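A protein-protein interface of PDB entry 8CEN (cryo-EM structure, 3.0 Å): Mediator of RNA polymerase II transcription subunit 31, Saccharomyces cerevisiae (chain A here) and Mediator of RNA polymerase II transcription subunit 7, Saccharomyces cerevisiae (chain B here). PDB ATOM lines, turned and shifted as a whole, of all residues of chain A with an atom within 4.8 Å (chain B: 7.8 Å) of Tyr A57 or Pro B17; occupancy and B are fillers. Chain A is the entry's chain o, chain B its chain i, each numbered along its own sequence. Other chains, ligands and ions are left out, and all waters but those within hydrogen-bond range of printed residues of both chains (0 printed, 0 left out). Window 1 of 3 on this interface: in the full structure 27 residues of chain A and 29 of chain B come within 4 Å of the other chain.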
ATOM      1  N   VAL A  25     -28.752  22.403 -11.113  1.00  0.00           N
ATOM      2  CA  VAL A  25     -27.771  21.453 -11.637  1.00  0.00           C
ATOM      3  C   VAL A  25     -26.544  21.389 -10.736  1.00  0.00           C
ATOM      4  O   VAL A  25     -26.048  20.300 -10.416  1.00  0.00           O
ATOM      5  CB  VAL A  25     -27.398  21.814 -13.087  1.00  0.00           C
ATOM      6  CG1 VAL A  25     -26.310  20.892 -13.606  1.00  0.00           C
ATOM      7  CG2 VAL A  25     -28.617  21.711 -13.976  1.00  0.00           C
ATOM      8  N   GLU A  26     -26.047  22.549 -10.293  1.00  0.00           N
ATOM      9  CA  GLU A  26     -24.882  22.561  -9.421  1.00  0.00           C
ATOM     10  C   GLU A  26     -25.204  21.984  -8.050  1.00  0.00           C
ATOM     11  O   GLU A  26     -24.345  21.343  -7.442  1.00  0.00           O
ATOM     12  CB  GLU A  26     -24.339  23.983  -9.305  1.00  0.00           C
ATOM     13  CG  GLU A  26     -23.468  24.374 -10.482  1.00  0.00           C
ATOM     14  CD  GLU A  26     -22.971  25.799 -10.411  1.00  0.00           C
ATOM     15  OE1 GLU A  26     -23.260  26.481  -9.409  1.00  0.00           O
ATOM     16  OE2 GLU A  26     -22.301  26.241 -11.366  1.00  0.00           O
ATOM     17  N   PHE A  29     -25.190  18.183  -8.560  1.00  0.00           N
ATOM     18  CA  PHE A  29     -23.829  17.676  -8.711  1.00  0.00           C
ATOM     19  C   PHE A  29     -23.045  17.747  -7.406  1.00  0.00           C
ATOM     20  O   PHE A  29     -22.298  16.816  -7.085  1.00  0.00           O
ATOM     21  CB  PHE A  29     -23.062  18.425  -9.795  1.00  0.00           C
ATOM     22  CG  PHE A  29     -21.666  17.903  -9.981  1.00  0.00           C
ATOM     23  CD1 PHE A  29     -21.454  16.604 -10.414  1.00  0.00           C
ATOM     24  CD2 PHE A  29     -20.570  18.681  -9.655  1.00  0.00           C
ATOM     25  CE1 PHE A  29     -20.174  16.109 -10.566  1.00  0.00           C
ATOM     26  CE2 PHE A  29     -19.287  18.192  -9.801  1.00  0.00           C
ATOM     27  CZ  PHE A  29     -19.090  16.903 -10.257  1.00  0.00           C
ATOM     28  N   ASN A  53      -9.947  21.622 -15.365  1.00  0.00           N
ATOM     29  CA  ASN A  53     -11.319  22.112 -15.323  1.00  0.00           C
ATOM     30  C   ASN A  53     -12.061  21.569 -14.108  1.00  0.00           C
ATOM     31  O   ASN A  53     -12.784  22.310 -13.435  1.00  0.00           O
ATOM     32  CB  ASN A  53     -12.052  21.721 -16.605  1.00  0.00           C
ATOM     33  CG  ASN A  53     -11.776  22.668 -17.754  1.00  0.00           C
ATOM     34  OD1 ASN A  53     -11.069  23.661 -17.600  1.00  0.00           O
ATOM     35  ND2 ASN A  53     -12.342  22.366 -18.915  1.00  0.00           N
ATOM     36  N   PHE A  54     -11.886  20.279 -13.808  1.00  0.00           N
ATOM     37  CA  PHE A  54     -12.544  19.689 -12.646  1.00  0.00           C
ATOM     38  C   PHE A  54     -11.974  20.239 -11.344  1.00  0.00           C
ATOM     39  O   PHE A  54     -12.715  20.439 -10.376  1.00  0.00           O
ATOM     40  CB  PHE A  54     -12.415  18.168 -12.681  1.00  0.00           C
ATOM     41  CG  PHE A  54     -13.485  17.454 -11.907  1.00  0.00           C
ATOM     42  CD1 PHE A  54     -14.820  17.623 -12.232  1.00  0.00           C
ATOM     43  CD2 PHE A  54     -13.158  16.629 -10.842  1.00  0.00           C
ATOM     44  CE1 PHE A  54     -15.809  16.972 -11.522  1.00  0.00           C
ATOM     45  CE2 PHE A  54     -14.143  15.972 -10.127  1.00  0.00           C
ATOM     46  CZ  PHE A  54     -15.471  16.146 -10.468  1.00  0.00           C
ATOM     47  N   LYS A  55     -10.659  20.480 -11.306  1.00  0.00           N
ATOM     48  CA  LYS A  55     -10.034  21.125 -10.154  1.00  0.00           C
ATOM     49  C   LYS A  55     -10.637  22.498  -9.894  1.00  0.00           C
ATOM     50  O   LYS A  55     -11.020  22.827  -8.761  1.00  0.00           O
ATOM     51  CB  LYS A  55      -8.529  21.253 -10.394  1.00  0.00           C
ATOM     52  CG  LYS A  55      -7.840  22.241  -9.466  1.00  0.00           C
ATOM     53  CD  LYS A  55      -6.353  22.327  -9.738  1.00  0.00           C
ATOM     54  CE  LYS A  55      -5.734  23.484  -8.975  1.00  0.00           C
ATOM     55  NZ  LYS A  55      -6.176  24.802  -9.509  1.00  0.00           N
ATOM     56  N   ASN A  56     -10.751  23.304 -10.949  1.00  0.00           N
ATOM     57  CA  ASN A  56     -11.271  24.652 -10.790  1.00  0.00           C
ATOM     58  C   ASN A  56     -12.759  24.629 -10.471  1.00  0.00           C
ATOM     59  O   ASN A  56     -13.245  25.481  -9.722  1.00  0.00           O
ATOM     60  CB  ASN A  56     -10.990  25.458 -12.053  1.00  0.00           C
ATOM     61  CG  ASN A  56      -9.512  25.732 -12.239  1.00  0.00           C
ATOM     62  OD1 ASN A  56      -8.801  26.037 -11.285  1.00  0.00           O
ATOM     63  ND2 ASN A  56      -9.043  25.629 -13.476  1.00  0.00           N
ATOM     64  N   TYR A  57     -13.484  23.636 -10.994  1.00  0.00           N
ATOM     65  CA  TYR A  57     -14.899  23.482 -10.678  1.00  0.00           C
ATOM     66  C   TYR A  57     -15.109  23.111  -9.215  1.00  0.00           C
ATOM     67  O   TYR A  57     -16.011  23.641  -8.561  1.00  0.00           O
ATOM     68  CB  TYR A  57     -15.515  22.416 -11.577  1.00  0.00           C
ATOM     69  CG  TYR A  57     -17.020  22.445 -11.624  1.00  0.00           C
ATOM     70  CD1 TYR A  57     -17.696  23.586 -12.030  1.00  0.00           C
ATOM     71  CD2 TYR A  57     -17.765  21.343 -11.239  1.00  0.00           C
ATOM     72  CE1 TYR A  57     -19.073  23.619 -12.077  1.00  0.00           C
ATOM     73  CE2 TYR A  57     -19.138  21.367 -11.284  1.00  0.00           C
ATOM     74  CZ  TYR A  57     -19.787  22.505 -11.700  1.00  0.00           C
ATOM     75  OH  TYR A  57     -21.158  22.522 -11.739  1.00  0.00           O
ATOM     76  N   LEU A  58     -14.295  22.191  -8.690  1.00  0.00           N
ATOM     77  CA  LEU A  58     -14.435  21.802  -7.291  1.00  0.00           C
ATOM     78  C   LEU A  58     -13.992  22.913  -6.351  1.00  0.00           C
ATOM     79  O   LEU A  58     -14.507  23.013  -5.232  1.00  0.00           O
ATOM     80  CB  LEU A  58     -13.648  20.523  -7.009  1.00  0.00           C
ATOM     81  CG  LEU A  58     -14.143  19.235  -7.669  1.00  0.00           C
ATOM     82  CD1 LEU A  58     -13.228  18.076  -7.311  1.00  0.00           C
ATOM     83  CD2 LEU A  58     -15.578  18.938  -7.272  1.00  0.00           C
ATOM     84  N   LYS A  59     -13.038  23.747  -6.773  1.00  0.00           N
ATOM     85  CA  LYS A  59     -12.722  24.934  -5.983  1.00  0.00           C
ATOM     86  C   LYS A  59     -13.867  25.945  -6.046  1.00  0.00           C
ATOM     87  O   LYS A  59     -14.161  26.624  -5.057  1.00  0.00           O
ATOM     88  CB  LYS A  59     -11.411  25.555  -6.471  1.00  0.00           C
ATOM     89  CG  LYS A  59     -10.921  26.782  -5.693  1.00  0.00           C
ATOM     90  CD  LYS A  59     -11.037  26.613  -4.178  1.00  0.00           C
ATOM     91  CE  LYS A  59      -9.977  25.669  -3.629  1.00  0.00           C
ATOM     92  NZ  LYS A  59     -10.277  25.261  -2.229  1.00  0.00           N
ATOM     93  N   TYR A  60     -14.520  26.051  -7.205  1.00  0.00           N
ATOM     94  CA  TYR A  60     -15.649  26.960  -7.372  1.00  0.00           C
ATOM     95  C   TYR A  60     -16.846  26.541  -6.530  1.00  0.00           C
ATOM     96  O   TYR A  60     -17.561  27.392  -5.991  1.00  0.00           O
ATOM     97  CB  TYR A  60     -16.026  27.022  -8.847  1.00  0.00           C
ATOM     98  CG  TYR A  60     -17.420  27.525  -9.132  1.00  0.00           C
ATOM     99  CD1 TYR A  60     -17.732  28.874  -9.042  1.00  0.00           C
ATOM    100  CD2 TYR A  60     -18.423  26.642  -9.510  1.00  0.00           C
ATOM    101  CE1 TYR A  60     -19.008  29.327  -9.316  1.00  0.00           C
ATOM    102  CE2 TYR A  60     -19.694  27.083  -9.783  1.00  0.00           C
ATOM    103  CZ  TYR A  60     -19.984  28.423  -9.686  1.00  0.00           C
ATOM    104  OH  TYR A  60     -21.259  28.853  -9.962  1.00  0.00           O
ATOM    105  N   LEU A  61     -17.077  25.239  -6.401  1.00  0.00           N
ATOM    106  CA  LEU A  61     -18.227  24.701  -5.668  1.00  0.00           C
ATOM    107  C   LEU A  61     -18.127  24.888  -4.149  1.00  0.00           C
ATOM    108  O   LEU A  61     -18.989  24.364  -3.434  1.00  0.00           O
ATOM    109  CB  LEU A  61     -18.412  23.220  -5.999  1.00  0.00           C
ATOM    110  CG  LEU A  61     -18.979  22.901  -7.385  1.00  0.00           C
ATOM    111  CD1 LEU A  61     -19.101  21.402  -7.589  1.00  0.00           C
ATOM    112  CD2 LEU A  61     -20.321  23.580  -7.595  1.00  0.00           C
ATOM    113  N   PRO B  14     -24.681   9.865 -14.313  1.00  0.00           N
ATOM    114  CA  PRO B  14     -24.621  11.048 -15.166  1.00  0.00           C
ATOM    115  C   PRO B  14     -23.239  11.673 -15.128  1.00  0.00           C
ATOM    116  O   PRO B  14     -22.514  11.549 -14.126  1.00  0.00           O
ATOM    117  CB  PRO B  14     -25.676  11.985 -14.549  1.00  0.00           C
ATOM    118  CG  PRO B  14     -26.557  11.097 -13.740  1.00  0.00           C
ATOM    119  CD  PRO B  14     -25.664  10.016 -13.228  1.00  0.00           C
ATOM    120  N   PRO B  15     -22.826  12.348 -16.196  1.00  0.00           N
ATOM    121  CA  PRO B  15     -21.525  13.022 -16.197  1.00  0.00           C
ATOM    122  C   PRO B  15     -21.566  14.290 -15.365  1.00  0.00           C
ATOM    123  O   PRO B  15     -22.646  14.719 -14.928  1.00  0.00           O
ATOM    124  CB  PRO B  15     -21.297  13.333 -17.685  1.00  0.00           C
ATOM    125  CG  PRO B  15     -22.654  13.408 -18.260  1.00  0.00           C
ATOM    126  CD  PRO B  15     -23.474  12.397 -17.517  1.00  0.00           C
ATOM    127  N   PRO B  16     -20.415  14.909 -15.104  1.00  0.00           N
ATOM    128  CA  PRO B  16     -20.400  16.241 -14.481  1.00  0.00           C
ATOM    129  C   PRO B  16     -21.071  17.275 -15.371  1.00  0.00           C
ATOM    130  O   PRO B  16     -21.240  17.044 -16.579  1.00  0.00           O
ATOM    131  CB  PRO B  16     -18.898  16.525 -14.322  1.00  0.00           C
ATOM    132  CG  PRO B  16     -18.303  15.188 -14.146  1.00  0.00           C
ATOM    133  CD  PRO B  16     -19.080  14.284 -15.063  1.00  0.00           C
ATOM    134  N   PRO B  17     -21.491  18.416 -14.809  1.00  0.00           N
ATOM    135  CA  PRO B  17     -22.224  19.397 -15.609  1.00  0.00           C
ATOM    136  C   PRO B  17     -21.348  20.003 -16.690  1.00  0.00           C
ATOM    137  O   PRO B  17     -20.132  20.182 -16.498  1.00  0.00           O
ATOM    138  CB  PRO B  17     -22.644  20.457 -14.573  1.00  0.00           C
ATOM    139  CG  PRO B  17     -22.584  19.768 -13.269  1.00  0.00           C
ATOM    140  CD  PRO B  17     -21.462  18.793 -13.384  1.00  0.00           C
ATOM    141  N   PRO B  18     -21.935  20.386 -17.832  1.00  0.00           N
ATOM    142  CA  PRO B  18     -21.138  20.993 -18.915  1.00  0.00           C
ATOM    143  C   PRO B  18     -20.466  22.290 -18.514  1.00  0.00           C
ATOM    144  O   PRO B  18     -19.498  22.702 -19.166  1.00  0.00           O
ATOM    145  CB  PRO B  18     -22.176  21.223 -20.022  1.00  0.00           C
ATOM    146  CG  PRO B  18     -23.477  21.321 -19.294  1.00  0.00           C
ATOM    147  CD  PRO B  18     -23.370  20.354 -18.156  1.00  0.00           C
ATOM    148  N   TYR B  19     -20.918  22.900 -17.413  1.00  0.00           N
ATOM    149  CA  TYR B  19     -20.314  24.104 -16.856  1.00  0.00           C
ATOM    150  C   TYR B  19     -18.834  23.907 -16.548  1.00  0.00           C
ATOM    151  O   TYR B  19     -18.069  24.881 -16.548  1.00  0.00           O
ATOM    152  CB  TYR B  19     -21.074  24.488 -15.584  1.00  0.00           C
ATOM    153  CG  TYR B  19     -22.554  24.746 -15.796  1.00  0.00           C
ATOM    154  CD1 TYR B  19     -23.045  25.177 -17.024  1.00  0.00           C
ATOM    155  CD2 TYR B  19     -23.469  24.487 -14.783  1.00  0.00           C
ATOM    156  CE1 TYR B  19     -24.395  25.385 -17.219  1.00  0.00           C
ATOM    157  CE2 TYR B  19     -24.821  24.687 -14.974  1.00  0.00           C
ATOM    158  CZ  TYR B  19     -25.277  25.142 -16.192  1.00  0.00           C
ATOM    159  OH  TYR B  19     -26.624  25.349 -16.386  1.00  0.00           O
ATOM    160  N   VAL B  20     -18.412  22.649 -16.321  1.00  0.00           N
ATOM    161  CA  VAL B  20     -17.004  22.322 -16.081  1.00  0.00           C
ATOM    162  C   VAL B  20     -16.102  22.826 -17.208  1.00  0.00           C
ATOM    163  O   VAL B  20     -14.956  23.226 -16.956  1.00  0.00           O
ATOM    164  CB  VAL B  20     -16.852  20.797 -15.860  1.00  0.00           C
ATOM    165  CG1 VAL B  20     -15.394  20.379 -15.722  1.00  0.00           C
ATOM    166  CG2 VAL B  20     -17.586  20.370 -14.613  1.00  0.00           C
ATOM    167  N   LYS B  21     -16.611  22.895 -18.447  1.00  0.00           N
ATOM    168  CA  LYS B  21     -15.740  23.336 -19.535  1.00  0.00           C
ATOM    169  C   LYS B  21     -15.383  24.817 -19.456  1.00  0.00           C
ATOM    170  O   LYS B  21     -14.455  25.244 -20.151  1.00  0.00           O
ATOM    171  CB  LYS B  21     -16.367  23.063 -20.905  1.00  0.00           C
ATOM    172  CG  LYS B  21     -17.527  23.970 -21.269  1.00  0.00           C
ATOM    173  CD  LYS B  21     -17.994  23.717 -22.691  1.00  0.00           C
ATOM    174  CE  LYS B  21     -18.398  25.011 -23.374  1.00  0.00           C
ATOM    175  NZ  LYS B  21     -18.926  24.773 -24.745  1.00  0.00           N
ATOM    176  N   PHE B  22     -16.077  25.609 -18.636  1.00  0.00           N
ATOM    177  CA  PHE B  22     -15.784  27.034 -18.560  1.00  0.00           C
ATOM    178  C   PHE B  22     -14.686  27.385 -17.564  1.00  0.00           C
ATOM    179  O   PHE B  22     -14.222  28.531 -17.562  1.00  0.00           O
ATOM    180  CB  PHE B  22     -17.047  27.823 -18.203  1.00  0.00           C
ATOM    181  CG  PHE B  22     -18.088  27.820 -19.282  1.00  0.00           C
ATOM    182  CD1 PHE B  22     -17.850  28.453 -20.490  1.00  0.00           C
ATOM    183  CD2 PHE B  22     -19.308  27.193 -19.087  1.00  0.00           C
ATOM    184  CE1 PHE B  22     -18.806  28.457 -21.487  1.00  0.00           C
ATOM    185  CE2 PHE B  22     -20.268  27.193 -20.079  1.00  0.00           C
ATOM    186  CZ  PHE B  22     -20.016  27.827 -21.280  1.00  0.00           C
ATOM    187  N   PHE B  23     -14.254  26.444 -16.724  1.00  0.00           N
ATOM    188  CA  PHE B  23     -13.395  26.774 -15.585  1.00  0.00           C
ATOM    189  C   PHE B  23     -11.937  26.481 -15.924  1.00  0.00           C
ATOM    190  O   PHE B  23     -11.334  25.512 -15.462  1.00  0.00           O
ATOM    191  CB  PHE B  23     -13.851  26.018 -14.346  1.00  0.00           C
ATOM    192  CG  PHE B  23     -15.114  26.558 -13.756  1.00  0.00           C
ATOM    193  CD1 PHE B  23     -16.344  26.120 -14.211  1.00  0.00           C
ATOM    194  CD2 PHE B  23     -15.073  27.528 -12.774  1.00  0.00           C
ATOM    195  CE1 PHE B  23     -17.509  26.624 -13.684  1.00  0.00           C
ATOM    196  CE2 PHE B  23     -16.235  28.037 -12.244  1.00  0.00           C
ATOM    197  CZ  PHE B  23     -17.455  27.581 -12.697  1.00  0.00           C
ATOM    198  N   THR B  24     -11.355  27.369 -16.723  1.00  0.00           N
ATOM    199  CA  THR B  24      -9.966  27.271 -17.139  1.00  0.00           C
ATOM    200  C   THR B  24      -9.122  28.298 -16.393  1.00  0.00           C
ATOM    201  O   THR B  24      -9.637  29.157 -15.669  1.00  0.00           O
ATOM    202  CB  THR B  24      -9.836  27.474 -18.651  1.00  0.00           C
ATOM    203  OG1 THR B  24     -10.175  28.826 -18.980  1.00  0.00           O
ATOM    204  CG2 THR B  24     -10.768  26.533 -19.392  1.00  0.00           C
ATOM    205  N   LEU B  28     -10.241  31.921 -14.955  1.00  0.00           N
ATOM    206  CA  LEU B  28     -10.003  32.287 -13.561  1.00  0.00           C
ATOM    207  C   LEU B  28      -9.164  33.553 -13.439  1.00  0.00           C
ATOM    208  O   LEU B  28      -9.372  34.344 -12.516  1.00  0.00           O
ATOM    209  CB  LEU B  28      -9.336  31.144 -12.803  1.00  0.00           C
ATOM    210  CG  LEU B  28     -10.234  30.023 -12.294  1.00  0.00           C
ATOM    211  CD1 LEU B  28      -9.432  29.170 -11.352  1.00  0.00           C
ATOM    212  CD2 LEU B  28     -11.456  30.580 -11.589  1.00  0.00           C
ATOM    213  N   TYR B  64     -20.597  32.092 -15.647  1.00  0.00           N
ATOM    214  CA  TYR B  64     -20.687  30.768 -15.052  1.00  0.00           C
ATOM    215  C   TYR B  64     -19.676  30.563 -13.934  1.00  0.00           C
ATOM    216  O   TYR B  64     -19.817  29.611 -13.162  1.00  0.00           O
ATOM    217  CB  TYR B  64     -20.502  29.691 -16.121  1.00  0.00           C
ATOM    218  CG  TYR B  64     -21.636  29.628 -17.119  1.00  0.00           C
ATOM    219  CD1 TYR B  64     -21.643  30.443 -18.244  1.00  0.00           C
ATOM    220  CD2 TYR B  64     -22.707  28.767 -16.928  1.00  0.00           C
ATOM    221  CE1 TYR B  64     -22.678  30.393 -19.155  1.00  0.00           C
ATOM    222  CE2 TYR B  64     -23.747  28.713 -17.834  1.00  0.00           C
ATOM    223  CZ  TYR B  64     -23.727  29.525 -18.945  1.00  0.00           C
ATOM    224  OH  TYR B  64     -24.761  29.472 -19.850  1.00  0.00           O
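Of chain B, only Pro B17 (3.5 Å), Val B20 (3.5 Å) and Phe B23 (3.5 Å) come within 4 Å of Tyr A57. Printed residues of chain A within 4 Å of Pro B17: Val A25, Phe A29 and Tyr A57. Of the printed residues of chain A, Val B20 touches Asn A53 (3.3 Å), Phe A54 (3.997 Å) and Tyr A57 (3.5 Å). Of the printed residues of chain A, Phe B23 touches Asn A53, Asn A56, Tyr A57 and Tyr A60. Of the printed residues of chain A, Thr B24 touches Asn A53 and Asn A56. Leu A58 touches none of the printed residues of chain B. The nearest printed residue of chain A that does not touch Pro B17 is Glu A26 (5.3 Å).
Hydrophobic or aromatic side chains of chain B that line the printed part of chain A: Pro B16, Pro B17, Val B20, Phe B23 and Leu B28. Of the 12 printed residues of chain A, 7 touch a printed residue of chain B. Among the printed residues, 16 pairs touch across the chains. Among the printed residues, no Asp or Glu carboxylate lies within 4 Å of a Lys or Arg side-chain nitrogen of the other chain.
NZ of Lys A55 lies within hydrogen-bond range of OD1 of Asn A56, 3.4 Å away. The side-chain carboxylate of Glu A26 sits at hydrogen-bond distance from the side-chain hydroxyl of Tyr A60, at 3.1 Å.
Among the printed residues, merely in contact across the chains: Val A25 with Pro B17, Phe A29 with Pro B16, Phe A29 with Pro B17, Asn A53 with Lys B21, Asn A53 with Thr B24, Phe A54 with Val B20, Asn A56 with Thr B24, Asn A56 with Leu B28, Tyr A57 with Pro B17, Tyr A57 with Val B20, Tyr A57 with Phe B23, Tyr A60 with Phe B23 and Tyr A60 with Tyr B64.
The side-chain amide nitrogen (ND2) of Asn A53 sits close to the backbone carbonyl oxygen (O) of Val B20, 3.4 Å away. The side-chain amide oxygen (OD1) of Asn A53 sits close to the backbone carbonyl oxygen (O) of Phe B23. ND2 of Asn A56 sits at hydrogen-bond distance from O of Phe B23 (3.0 Å).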
